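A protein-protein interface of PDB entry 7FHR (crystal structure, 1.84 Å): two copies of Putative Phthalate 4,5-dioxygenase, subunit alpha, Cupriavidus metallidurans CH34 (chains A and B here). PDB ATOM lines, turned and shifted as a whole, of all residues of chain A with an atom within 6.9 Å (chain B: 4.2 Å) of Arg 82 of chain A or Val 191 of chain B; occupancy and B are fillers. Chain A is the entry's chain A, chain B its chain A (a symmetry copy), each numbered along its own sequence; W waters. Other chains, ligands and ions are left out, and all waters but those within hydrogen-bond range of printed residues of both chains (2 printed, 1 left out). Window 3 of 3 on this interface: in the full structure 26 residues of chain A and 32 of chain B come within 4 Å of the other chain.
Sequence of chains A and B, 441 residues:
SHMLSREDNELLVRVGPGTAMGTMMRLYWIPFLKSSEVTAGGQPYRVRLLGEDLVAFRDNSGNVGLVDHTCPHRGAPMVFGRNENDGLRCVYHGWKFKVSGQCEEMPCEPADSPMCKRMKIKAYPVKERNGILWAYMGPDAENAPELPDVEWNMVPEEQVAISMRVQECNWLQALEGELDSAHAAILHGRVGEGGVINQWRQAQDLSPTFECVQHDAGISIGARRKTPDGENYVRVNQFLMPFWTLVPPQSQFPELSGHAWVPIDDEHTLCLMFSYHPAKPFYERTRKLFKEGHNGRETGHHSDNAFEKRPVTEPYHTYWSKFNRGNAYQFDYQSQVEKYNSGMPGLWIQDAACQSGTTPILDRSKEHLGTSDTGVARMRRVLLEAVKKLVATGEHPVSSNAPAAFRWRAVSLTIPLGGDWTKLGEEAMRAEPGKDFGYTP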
ATOM      1  N   GLY A  41     -31.421  15.988 -10.500  1.00  0.00           N
ATOM      2  CA  GLY A  41     -30.908  16.530 -11.744  1.00  0.00           C
ATOM      3  C   GLY A  41     -29.478  17.066 -11.677  1.00  0.00           C
ATOM      4  O   GLY A  41     -29.014  17.661 -12.639  1.00  0.00           O
ATOM      5  N   GLY A  42     -28.768  16.840 -10.565  1.00  0.00           N
ATOM      6  CA  GLY A  42     -27.415  17.350 -10.394  1.00  0.00           C
ATOM      7  C   GLY A  42     -26.344  16.364 -10.866  1.00  0.00           C
ATOM      8  O   GLY A  42     -26.609  15.387 -11.586  1.00  0.00           O
ATOM      9  N   PRO A  44     -23.870  13.328 -11.264  1.00  0.00           N
ATOM     10  CA  PRO A  44     -23.790  11.932 -10.826  1.00  0.00           C
ATOM     11  C   PRO A  44     -22.569  11.781  -9.908  1.00  0.00           C
ATOM     12  O   PRO A  44     -21.717  12.664  -9.878  1.00  0.00           O
ATOM     13  CB  PRO A  44     -23.524  11.129 -12.119  1.00  0.00           C
ATOM     14  CG  PRO A  44     -23.824  12.095 -13.235  1.00  0.00           C
ATOM     15  CD  PRO A  44     -23.561  13.494 -12.691  1.00  0.00           C
ATOM     16  N   PHE A  57     -27.099   8.482  -9.494  1.00  0.00           N
ATOM     17  CA  PHE A  57     -27.591   9.813  -9.848  1.00  0.00           C
ATOM     18  C   PHE A  57     -29.025   9.915  -9.335  1.00  0.00           C
ATOM     19  O   PHE A  57     -29.731   8.908  -9.276  1.00  0.00           O
ATOM     20  CB  PHE A  57     -27.503  10.100 -11.358  1.00  0.00           C
ATOM     21  CG  PHE A  57     -28.443   9.280 -12.219  1.00  0.00           C
ATOM     22  CD1 PHE A  57     -28.181   7.943 -12.491  1.00  0.00           C
ATOM     23  CD2 PHE A  57     -29.603   9.836 -12.755  1.00  0.00           C
ATOM     24  CE1 PHE A  57     -29.062   7.176 -13.245  1.00  0.00           C
ATOM     25  CE2 PHE A  57     -30.476   9.078 -13.530  1.00  0.00           C
ATOM     26  CZ  PHE A  57     -30.206   7.742 -13.768  1.00  0.00           C
ATOM     27  N   MET A  78     -19.983   6.945 -17.786  1.00  0.00           N
ATOM     28  CA  MET A  78     -21.301   7.442 -17.430  1.00  0.00           C
ATOM     29  C   MET A  78     -21.225   8.598 -16.416  1.00  0.00           C
ATOM     30  O   MET A  78     -22.171   9.399 -16.340  1.00  0.00           O
ATOM     31  CB  MET A  78     -22.193   6.312 -16.883  1.00  0.00           C
ATOM     32  CG  MET A  78     -22.655   5.282 -17.946  1.00  0.00           C
ATOM     33  SD  MET A  78     -23.353   6.016 -19.479  1.00  0.00           S
ATOM     34  CE  MET A  78     -24.733   6.928 -18.772  1.00  0.00           C
ATOM     35  N   VAL A  79     -20.107   8.770 -15.688  1.00  0.00           N
ATOM     36  CA  VAL A  79     -20.078   9.893 -14.741  1.00  0.00           C
ATOM     37  C   VAL A  79     -20.068  11.237 -15.504  1.00  0.00           C
ATOM     38  O   VAL A  79     -20.409  12.263 -14.939  1.00  0.00           O
ATOM     39  CB  VAL A  79     -18.891   9.765 -13.763  1.00  0.00           C
ATOM     40  CG1 VAL A  79     -17.533   9.964 -14.444  1.00  0.00           C
ATOM     41  CG2 VAL A  79     -19.062  10.669 -12.548  1.00  0.00           C
ATOM     42  N   PHE A  80     -19.762  11.235 -16.808  1.00  0.00           N
ATOM     43  CA  PHE A  80     -19.750  12.455 -17.595  1.00  0.00           C
ATOM     44  C   PHE A  80     -21.088  12.667 -18.306  1.00  0.00           C
ATOM     45  O   PHE A  80     -21.210  13.601 -19.109  1.00  0.00           O
ATOM     46  CB  PHE A  80     -18.597  12.415 -18.604  1.00  0.00           C
ATOM     47  CG  PHE A  80     -17.217  12.336 -18.003  1.00  0.00           C
ATOM     48  CD1 PHE A  80     -16.884  13.054 -16.850  1.00  0.00           C
ATOM     49  CD2 PHE A  80     -16.230  11.548 -18.595  1.00  0.00           C
ATOM     50  CE1 PHE A  80     -15.583  13.014 -16.351  1.00  0.00           C
ATOM     51  CE2 PHE A  80     -14.940  11.505 -18.092  1.00  0.00           C
ATOM     52  CZ  PHE A  80     -14.618  12.232 -16.959  1.00  0.00           C
ATOM     53  N   GLY A  81     -22.093  11.828 -17.997  1.00  0.00           N
ATOM     54  CA  GLY A  81     -23.351  11.900 -18.698  1.00  0.00           C
ATOM     55  C   GLY A  81     -24.171  13.105 -18.222  1.00  0.00           C
ATOM     56  O   GLY A  81     -23.852  13.734 -17.208  1.00  0.00           O
ATOM     57  N   ARG A  82     -25.244  13.381 -18.960  1.00  0.00           N
ATOM     58  CA  ARG A  82     -26.087  14.528 -18.659  1.00  0.00           C
ATOM     59  C   ARG A  82     -27.289  14.002 -17.897  1.00  0.00           C
ATOM     60  O   ARG A  82     -27.997  13.127 -18.401  1.00  0.00           O
ATOM     61  CB  ARG A  82     -26.578  15.194 -19.952  1.00  0.00           C
ATOM     62  CG  ARG A  82     -25.474  15.772 -20.809  1.00  0.00           C
ATOM     63  CD  ARG A  82     -26.065  16.437 -22.043  1.00  0.00           C
ATOM     64  NE  ARG A  82     -26.960  17.531 -21.639  1.00  0.00           N
ATOM     65  CZ  ARG A  82     -26.528  18.746 -21.288  1.00  0.00           C
ATOM     66  NH1 ARG A  82     -25.233  19.016 -21.305  1.00  0.00           N
ATOM     67  NH2 ARG A  82     -27.389  19.678 -20.916  1.00  0.00           N
ATOM     68  N   ASN A  83     -27.459  14.498 -16.671  1.00  0.00           N
ATOM     69  CA  ASN A  83     -28.562  14.103 -15.810  1.00  0.00           C
ATOM     70  C   ASN A  83     -29.671  15.125 -16.027  1.00  0.00           C
ATOM     71  O   ASN A  83     -29.545  16.255 -15.559  1.00  0.00           O
ATOM     72  CB  ASN A  83     -28.142  14.202 -14.339  1.00  0.00           C
ATOM     73  CG  ASN A  83     -29.162  13.657 -13.346  1.00  0.00           C
ATOM     74  OD1 ASN A  83     -30.238  13.147 -13.707  1.00  0.00           O
ATOM     75  ND2 ASN A  83     -28.797  13.696 -12.074  1.00  0.00           N
ATOM     76  N   GLU A  84     -30.700  14.765 -16.794  1.00  0.00           N
ATOM     77  CA  GLU A  84     -31.780  15.698 -17.120  1.00  0.00           C
ATOM     78  C   GLU A  84     -32.939  14.949 -17.735  1.00  0.00           C
ATOM     79  O   GLU A  84     -32.760  13.847 -18.253  1.00  0.00           O
ATOM     80  CB  GLU A  84     -31.366  16.783 -18.120  1.00  0.00           C
ATOM     81  CG  GLU A  84     -30.857  16.275 -19.446  1.00  0.00           C
ATOM     82  CD  GLU A  84     -30.065  17.315 -20.210  1.00  0.00           C
ATOM     83  OE1 GLU A  84     -29.702  17.026 -21.357  1.00  0.00           O
ATOM     84  OE2 GLU A  84     -29.814  18.430 -19.662  1.00  0.00           O
ATOM     85  N   ASN A  85     -34.130  15.569 -17.652  1.00  0.00           N
ATOM     86  CA  ASN A  85     -35.345  14.970 -18.174  1.00  0.00           C
ATOM     87  C   ASN A  85     -35.466  13.540 -17.652  1.00  0.00           C
ATOM     88  O   ASN A  85     -35.833  12.644 -18.405  1.00  0.00           O
ATOM     89  CB  ASN A  85     -35.396  15.004 -19.711  1.00  0.00           C
ATOM     90  CG  ASN A  85     -35.397  16.411 -20.263  1.00  0.00           C
ATOM     91  OD1 ASN A  85     -36.300  17.189 -19.966  1.00  0.00           O
ATOM     92  ND2 ASN A  85     -34.397  16.759 -21.060  1.00  0.00           N
ATOM     93  N   GLY A  87     -33.398  11.141 -16.571  1.00  0.00           N
ATOM     94  CA  GLY A  87     -32.517  10.117 -17.125  1.00  0.00           C
ATOM     95  C   GLY A  87     -31.069  10.587 -17.081  1.00  0.00           C
ATOM     96  O   GLY A  87     -30.789  11.747 -16.777  1.00  0.00           O
ATOM     97  N   LEU A  88     -30.152   9.659 -17.337  1.00  0.00           N
ATOM     98  CA  LEU A  88     -28.746  10.015 -17.461  1.00  0.00           C
ATOM     99  C   LEU A  88     -28.333   9.618 -18.873  1.00  0.00           C
ATOM    100  O   LEU A  88     -28.526   8.485 -19.281  1.00  0.00           O
ATOM    101  CB  LEU A  88     -27.946   9.205 -16.428  1.00  0.00           C
ATOM    102  CG  LEU A  88     -26.434   9.446 -16.411  1.00  0.00           C
ATOM    103  CD1 LEU A  88     -26.151  10.866 -15.915  1.00  0.00           C
ATOM    104  CD2 LEU A  88     -25.733   8.401 -15.530  1.00  0.00           C
ATOM    105  N   ARG A  89     -27.782  10.568 -19.629  1.00  0.00           N
ATOM    106  CA  ARG A  89     -27.569  10.363 -21.045  1.00  0.00           C
ATOM    107  C   ARG A  89     -26.072  10.418 -21.318  1.00  0.00           C
ATOM    108  O   ARG A  89     -25.441  11.421 -21.014  1.00  0.00           O
ATOM    109  CB  ARG A  89     -28.265  11.468 -21.850  1.00  0.00           C
ATOM    110  CG  ARG A  89     -28.149  11.240 -23.346  1.00  0.00           C
ATOM    111  CD  ARG A  89     -28.486  12.435 -24.229  1.00  0.00           C
ATOM    112  NE  ARG A  89     -29.870  12.866 -24.120  1.00  0.00           N
ATOM    113  CZ  ARG A  89     -30.903  12.368 -24.787  1.00  0.00           C
ATOM    114  NH1 ARG A  89     -30.746  11.365 -25.640  1.00  0.00           N
ATOM    115  NH2 ARG A  89     -32.113  12.882 -24.581  1.00  0.00           N
ATOM    116  N   CYS A  90     -25.526   9.349 -21.927  1.00  0.00           N
ATOM    117  CA  CYS A  90     -24.118   9.310 -22.313  1.00  0.00           C
ATOM    118  C   CYS A  90     -23.892  10.343 -23.418  1.00  0.00           C
ATOM    119  O   CYS A  90     -24.677  10.436 -24.363  1.00  0.00           O
ATOM    120  CB  CYS A  90     -23.770   7.913 -22.840  1.00  0.00           C
ATOM    121  SG  CYS A  90     -22.070   7.786 -23.414  1.00  0.00           S
ATOM    122  N   VAL A  91     -22.815  11.129 -23.312  1.00  0.00           N
ATOM    123  CA  VAL A  91     -22.645  12.269 -24.219  1.00  0.00           C
ATOM    124  C   VAL A  91     -22.025  11.804 -25.526  1.00  0.00           C
ATOM    125  O   VAL A  91     -21.946  12.579 -26.481  1.00  0.00           O
ATOM    126  CB  VAL A  91     -21.739  13.369 -23.610  1.00  0.00           C
ATOM    127  CG1 VAL A  91     -22.468  14.158 -22.524  1.00  0.00           C
ATOM    128  CG2 VAL A  91     -20.463  12.787 -23.054  1.00  0.00           C
ATOM    129  N   LYS A  96     -29.793   7.297 -23.549  1.00  0.00           N
ATOM    130  CA  LYS A  96     -30.326   7.827 -22.302  1.00  0.00           C
ATOM    131  C   LYS A  96     -31.007   6.717 -21.499  1.00  0.00           C
ATOM    132  O   LYS A  96     -31.794   5.945 -22.041  1.00  0.00           O
ATOM    133  CB  LYS A  96     -31.371   8.910 -22.565  1.00  0.00           C
ATOM    134  CG  LYS A  96     -31.983   9.521 -21.316  1.00  0.00           C
ATOM    135  CD  LYS A  96     -33.098  10.488 -21.689  1.00  0.00           C
ATOM    136  CE  LYS A  96     -33.579  11.350 -20.528  1.00  0.00           C
ATOM    137  NZ  LYS A  96     -35.058  11.442 -20.499  1.00  0.00           N
ATOM    138  N   ARG B 190     -23.783  22.391 -28.487  1.00  0.00           N
ATOM    139  CA  ARG B 190     -24.131  23.381 -27.478  1.00  0.00           C
ATOM    140  C   ARG B 190     -25.524  23.129 -26.879  1.00  0.00           C
ATOM    141  O   ARG B 190     -26.419  22.623 -27.562  1.00  0.00           O
ATOM    142  CB  ARG B 190     -24.118  24.760 -28.135  1.00  0.00           C
ATOM    143  CG  ARG B 190     -22.875  25.036 -28.960  1.00  0.00           C
ATOM    144  CD  ARG B 190     -21.815  25.772 -28.161  1.00  0.00           C
ATOM    145  NE  ARG B 190     -22.004  27.215 -28.288  1.00  0.00           N
ATOM    146  CZ  ARG B 190     -22.427  28.041 -27.320  1.00  0.00           C
ATOM    147  NH1 ARG B 190     -22.700  27.589 -26.103  1.00  0.00           N
ATOM    148  NH2 ARG B 190     -22.563  29.332 -27.574  1.00  0.00           N
ATOM    149  N   VAL B 191     -25.701  23.477 -25.589  1.00  0.00           N
ATOM    150  CA  VAL B 191     -26.964  23.241 -24.909  1.00  0.00           C
ATOM    151  C   VAL B 191     -28.037  24.110 -25.584  1.00  0.00           C
ATOM    152  O   VAL B 191     -27.748  25.244 -25.994  1.00  0.00           O
ATOM    153  CB  VAL B 191     -26.841  23.498 -23.391  1.00  0.00           C
ATOM    154  CG1 VAL B 191     -28.173  23.405 -22.655  1.00  0.00           C
ATOM    155  CG2 VAL B 191     -25.836  22.561 -22.733  1.00  0.00           C
ATOM    156  N   GLY B 192     -29.250  23.548 -25.747  1.00  0.00           N
ATOM    157  CA  GLY B 192     -30.361  24.232 -26.400  1.00  0.00           C
ATOM    158  C   GLY B 192     -30.179  24.366 -27.915  1.00  0.00           C
ATOM    159  O   GLY B 192     -30.254  23.366 -28.632  1.00  0.00           O
ATOM    160  N   GLU B 193     -29.988  25.617 -28.383  1.00  0.00           N
ATOM    161  CA  GLU B 193     -29.642  25.946 -29.762  1.00  0.00           C
ATOM    162  C   GLU B 193     -28.114  25.952 -29.902  1.00  0.00           C
ATOM    163  O   GLU B 193     -27.653  25.888 -31.060  1.00  0.00           O
ATOM    164  CB  GLU B 193     -30.182  27.320 -30.188  1.00  0.00           C
ATOM    165  CG  GLU B 193     -31.633  27.311 -30.647  1.00  0.00           C
ATOM    166  CD  GLU B 193     -32.606  27.016 -29.517  1.00  0.00           C
ATOM    167  OE1 GLU B 193     -32.789  27.900 -28.655  1.00  0.00           O
ATOM    168  OE2 GLU B 193     -33.143  25.887 -29.473  1.00  0.00           O
ATOM    169  N   GLN B 336     -21.171  22.201 -18.552  1.00  0.00           N
ATOM    170  CA  GLN B 336     -22.038  21.205 -19.172  1.00  0.00           C
ATOM    171  C   GLN B 336     -23.492  21.639 -18.970  1.00  0.00           C
ATOM    172  O   GLN B 336     -24.309  21.482 -19.864  1.00  0.00           O
ATOM    173  CB  GLN B 336     -21.828  19.816 -18.541  1.00  0.00           C
ATOM    174  CG  GLN B 336     -22.632  18.707 -19.226  1.00  0.00           C
ATOM    175  CD  GLN B 336     -21.966  17.357 -19.009  1.00  0.00           C
ATOM    176  OE1 GLN B 336     -20.839  17.142 -19.454  1.00  0.00           O
ATOM    177  NE2 GLN B 336     -22.641  16.438 -18.334  1.00  0.00           N
ATOM    178  N   VAL B 337     -23.782  22.192 -17.784  1.00  0.00           N
ATOM    179  CA  VAL B 337     -25.119  22.678 -17.444  1.00  0.00           C
ATOM    180  C   VAL B 337     -25.465  23.867 -18.346  1.00  0.00           C
ATOM    181  O   VAL B 337     -26.550  23.907 -18.915  1.00  0.00           O
ATOM    182  CB  VAL B 337     -25.188  23.082 -15.959  1.00  0.00           C
ATOM    183  CG1 VAL B 337     -26.339  24.038 -15.667  1.00  0.00           C
ATOM    184  CG2 VAL B 337     -25.226  21.886 -15.029  1.00  0.00           C
ATOM    185  N   LYS B 339     -23.666  25.517 -21.130  1.00  0.00           N
ATOM    186  CA  LYS B 339     -23.261  25.885 -22.477  1.00  0.00           C
ATOM    187  C   LYS B 339     -22.984  24.689 -23.396  1.00  0.00           C
ATOM    188  O   LYS B 339     -23.315  24.771 -24.579  1.00  0.00           O
ATOM    189  CB  LYS B 339     -22.071  26.851 -22.463  1.00  0.00           C
ATOM    190  CG  LYS B 339     -22.467  28.322 -22.440  1.00  0.00           C
ATOM    191  CD  LYS B 339     -21.359  29.310 -22.812  1.00  0.00           C
ATOM    192  CE  LYS B 339     -20.546  28.883 -24.034  1.00  0.00           C
ATOM    193  NZ  LYS B 339     -19.667  29.968 -24.544  1.00  0.00           N
ATOM    194  N   TYR B 340     -22.370  23.608 -22.882  1.00  0.00           N
ATOM    195  CA  TYR B 340     -21.863  22.579 -23.787  1.00  0.00           C
ATOM    196  C   TYR B 340     -22.470  21.218 -23.466  1.00  0.00           C
ATOM    197  O   TYR B 340     -22.693  20.908 -22.296  1.00  0.00           O
ATOM    198  CB  TYR B 340     -20.340  22.531 -23.688  1.00  0.00           C
ATOM    199  CG  TYR B 340     -19.685  23.711 -24.359  1.00  0.00           C
ATOM    200  CD1 TYR B 340     -19.584  23.744 -25.740  1.00  0.00           C
ATOM    201  CD2 TYR B 340     -19.172  24.784 -23.636  1.00  0.00           C
ATOM    202  CE1 TYR B 340     -18.972  24.792 -26.402  1.00  0.00           C
ATOM    203  CE2 TYR B 340     -18.570  25.861 -24.280  1.00  0.00           C
ATOM    204  CZ  TYR B 340     -18.470  25.854 -25.667  1.00  0.00           C
ATOM    205  OH  TYR B 340     -17.879  26.849 -26.391  1.00  0.00           O
ATOM    206  N   ASN B 341     -22.801  20.443 -24.515  1.00  0.00           N
ATOM    207  CA  ASN B 341     -23.387  19.128 -24.273  1.00  0.00           C
ATOM    208  C   ASN B 341     -22.460  18.367 -23.332  1.00  0.00           C
ATOM    209  O   ASN B 341     -22.932  17.746 -22.382  1.00  0.00           O
ATOM    210  CB  ASN B 341     -23.688  18.342 -25.558  1.00  0.00           C
ATOM    211  CG  ASN B 341     -24.837  18.924 -26.363  1.00  0.00           C
ATOM    212  OD1 ASN B 341     -25.557  19.787 -25.866  1.00  0.00           O
ATOM    213  ND2 ASN B 341     -25.017  18.483 -27.600  1.00  0.00           N
HETATM  214  O   HOH W   1     -25.637  17.318 -16.835  1.00  0.00           O
HETATM  215  O   HOH W   2     -19.376  15.248 -20.687  1.00  0.00           O
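The side-chain amide nitrogen of Gln 336 of chain B lies within hydrogen-bond range of the backbone carbonyl oxygen of Phe 80 of chain A, 3.3 Å away.
NE2 of Gln 336 of chain B sits at hydrogen-bond distance from O of Gly 81 of chain A.
The guanidinium group (NH1) of Arg 82 of chain A lies within hydrogen-bond range of the backbone carbonyl oxygen (O) of Gln 336 of chain B (3.0 Å).
The guanidinium group (NH1) of Arg 82 of chain A sits at hydrogen-bond distance from the backbone carbonyl oxygen (O) of Tyr 340 of chain B.
The guanidinium group of Arg 82 of chain A is in hydrogen-bond range of the backbone carbonyl oxygen of Asn 341 of chain B (2.8 Å).
The guanidinium group (NE) of Arg 82 of chain A is in salt-bridge range of the side-chain carboxylate (OE1) of Glu 84 of chain A (2.8 Å).
The backbone NH (N) of Arg 82 of chain A is in hydrogen-bond range of the backbone carbonyl oxygen (O) of Arg 89 of chain A, at 2.8 Å.
O of Arg 190 of chain B sits close to OD1 of Asn 341 of chain B (3.4 Å).
O of Lys 339 of chain B sits at hydrogen-bond distance from N of Val 191 of chain B.
Among the printed residues, merely in contact across the chains: Arg 82 of chain A with Val 191 of chain B (3.7 Å) and Val 91 of chain A with Asn 341 of chain B (3.6 Å).
Of the printed residues of chain B, Phe 80 of chain A touches Gln 336.
Of the printed residues of chain B, Gly 81 of chain A touches Gln 336.
Arg 82 of chain A touches just these residues of chain B: Val 191, Gln 336, Tyr 340 and Asn 341.
Cys 90 of chain A touches none of the printed residues of chain B.
Val 191 of chain B touches one residue of chain A.
Of the printed residues of chain A, Gln 336 of chain B touches Phe 80 (3.3 Å), Gly 81 (3.2 Å) and Arg 82 (3.0 Å).
Of the printed residues of chain A, Asn 341 of chain B touches Arg 82 and Val 91.
The nearest printed residue of chain A that does not touch Gln 336 of chain B is Val 91 of chain A (4.6 Å).
Of the 9 printed residues of chain B, 4 touch a printed residue of chain A.
Hydrophobic or aromatic side chains of chain B within 4 Å of the printed part of chain A: Val 191.
Among the printed residues, no Asp or Glu carboxylate lies within 4 Å of a Lys or Arg side-chain nitrogen of the other chain.
No position is printed for both chains.
Water W2 bridges OE1 of Gln 336 of chain B (2.7 Å) and O of Phe 80 of chain A (2.9 Å).
Water W1 bridges the backbone NH (N) of Asn 83 of chain A (3.4 Å) and the side-chain amide nitrogen (NE2) of Gln 336 of chain B (3.5 Å).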
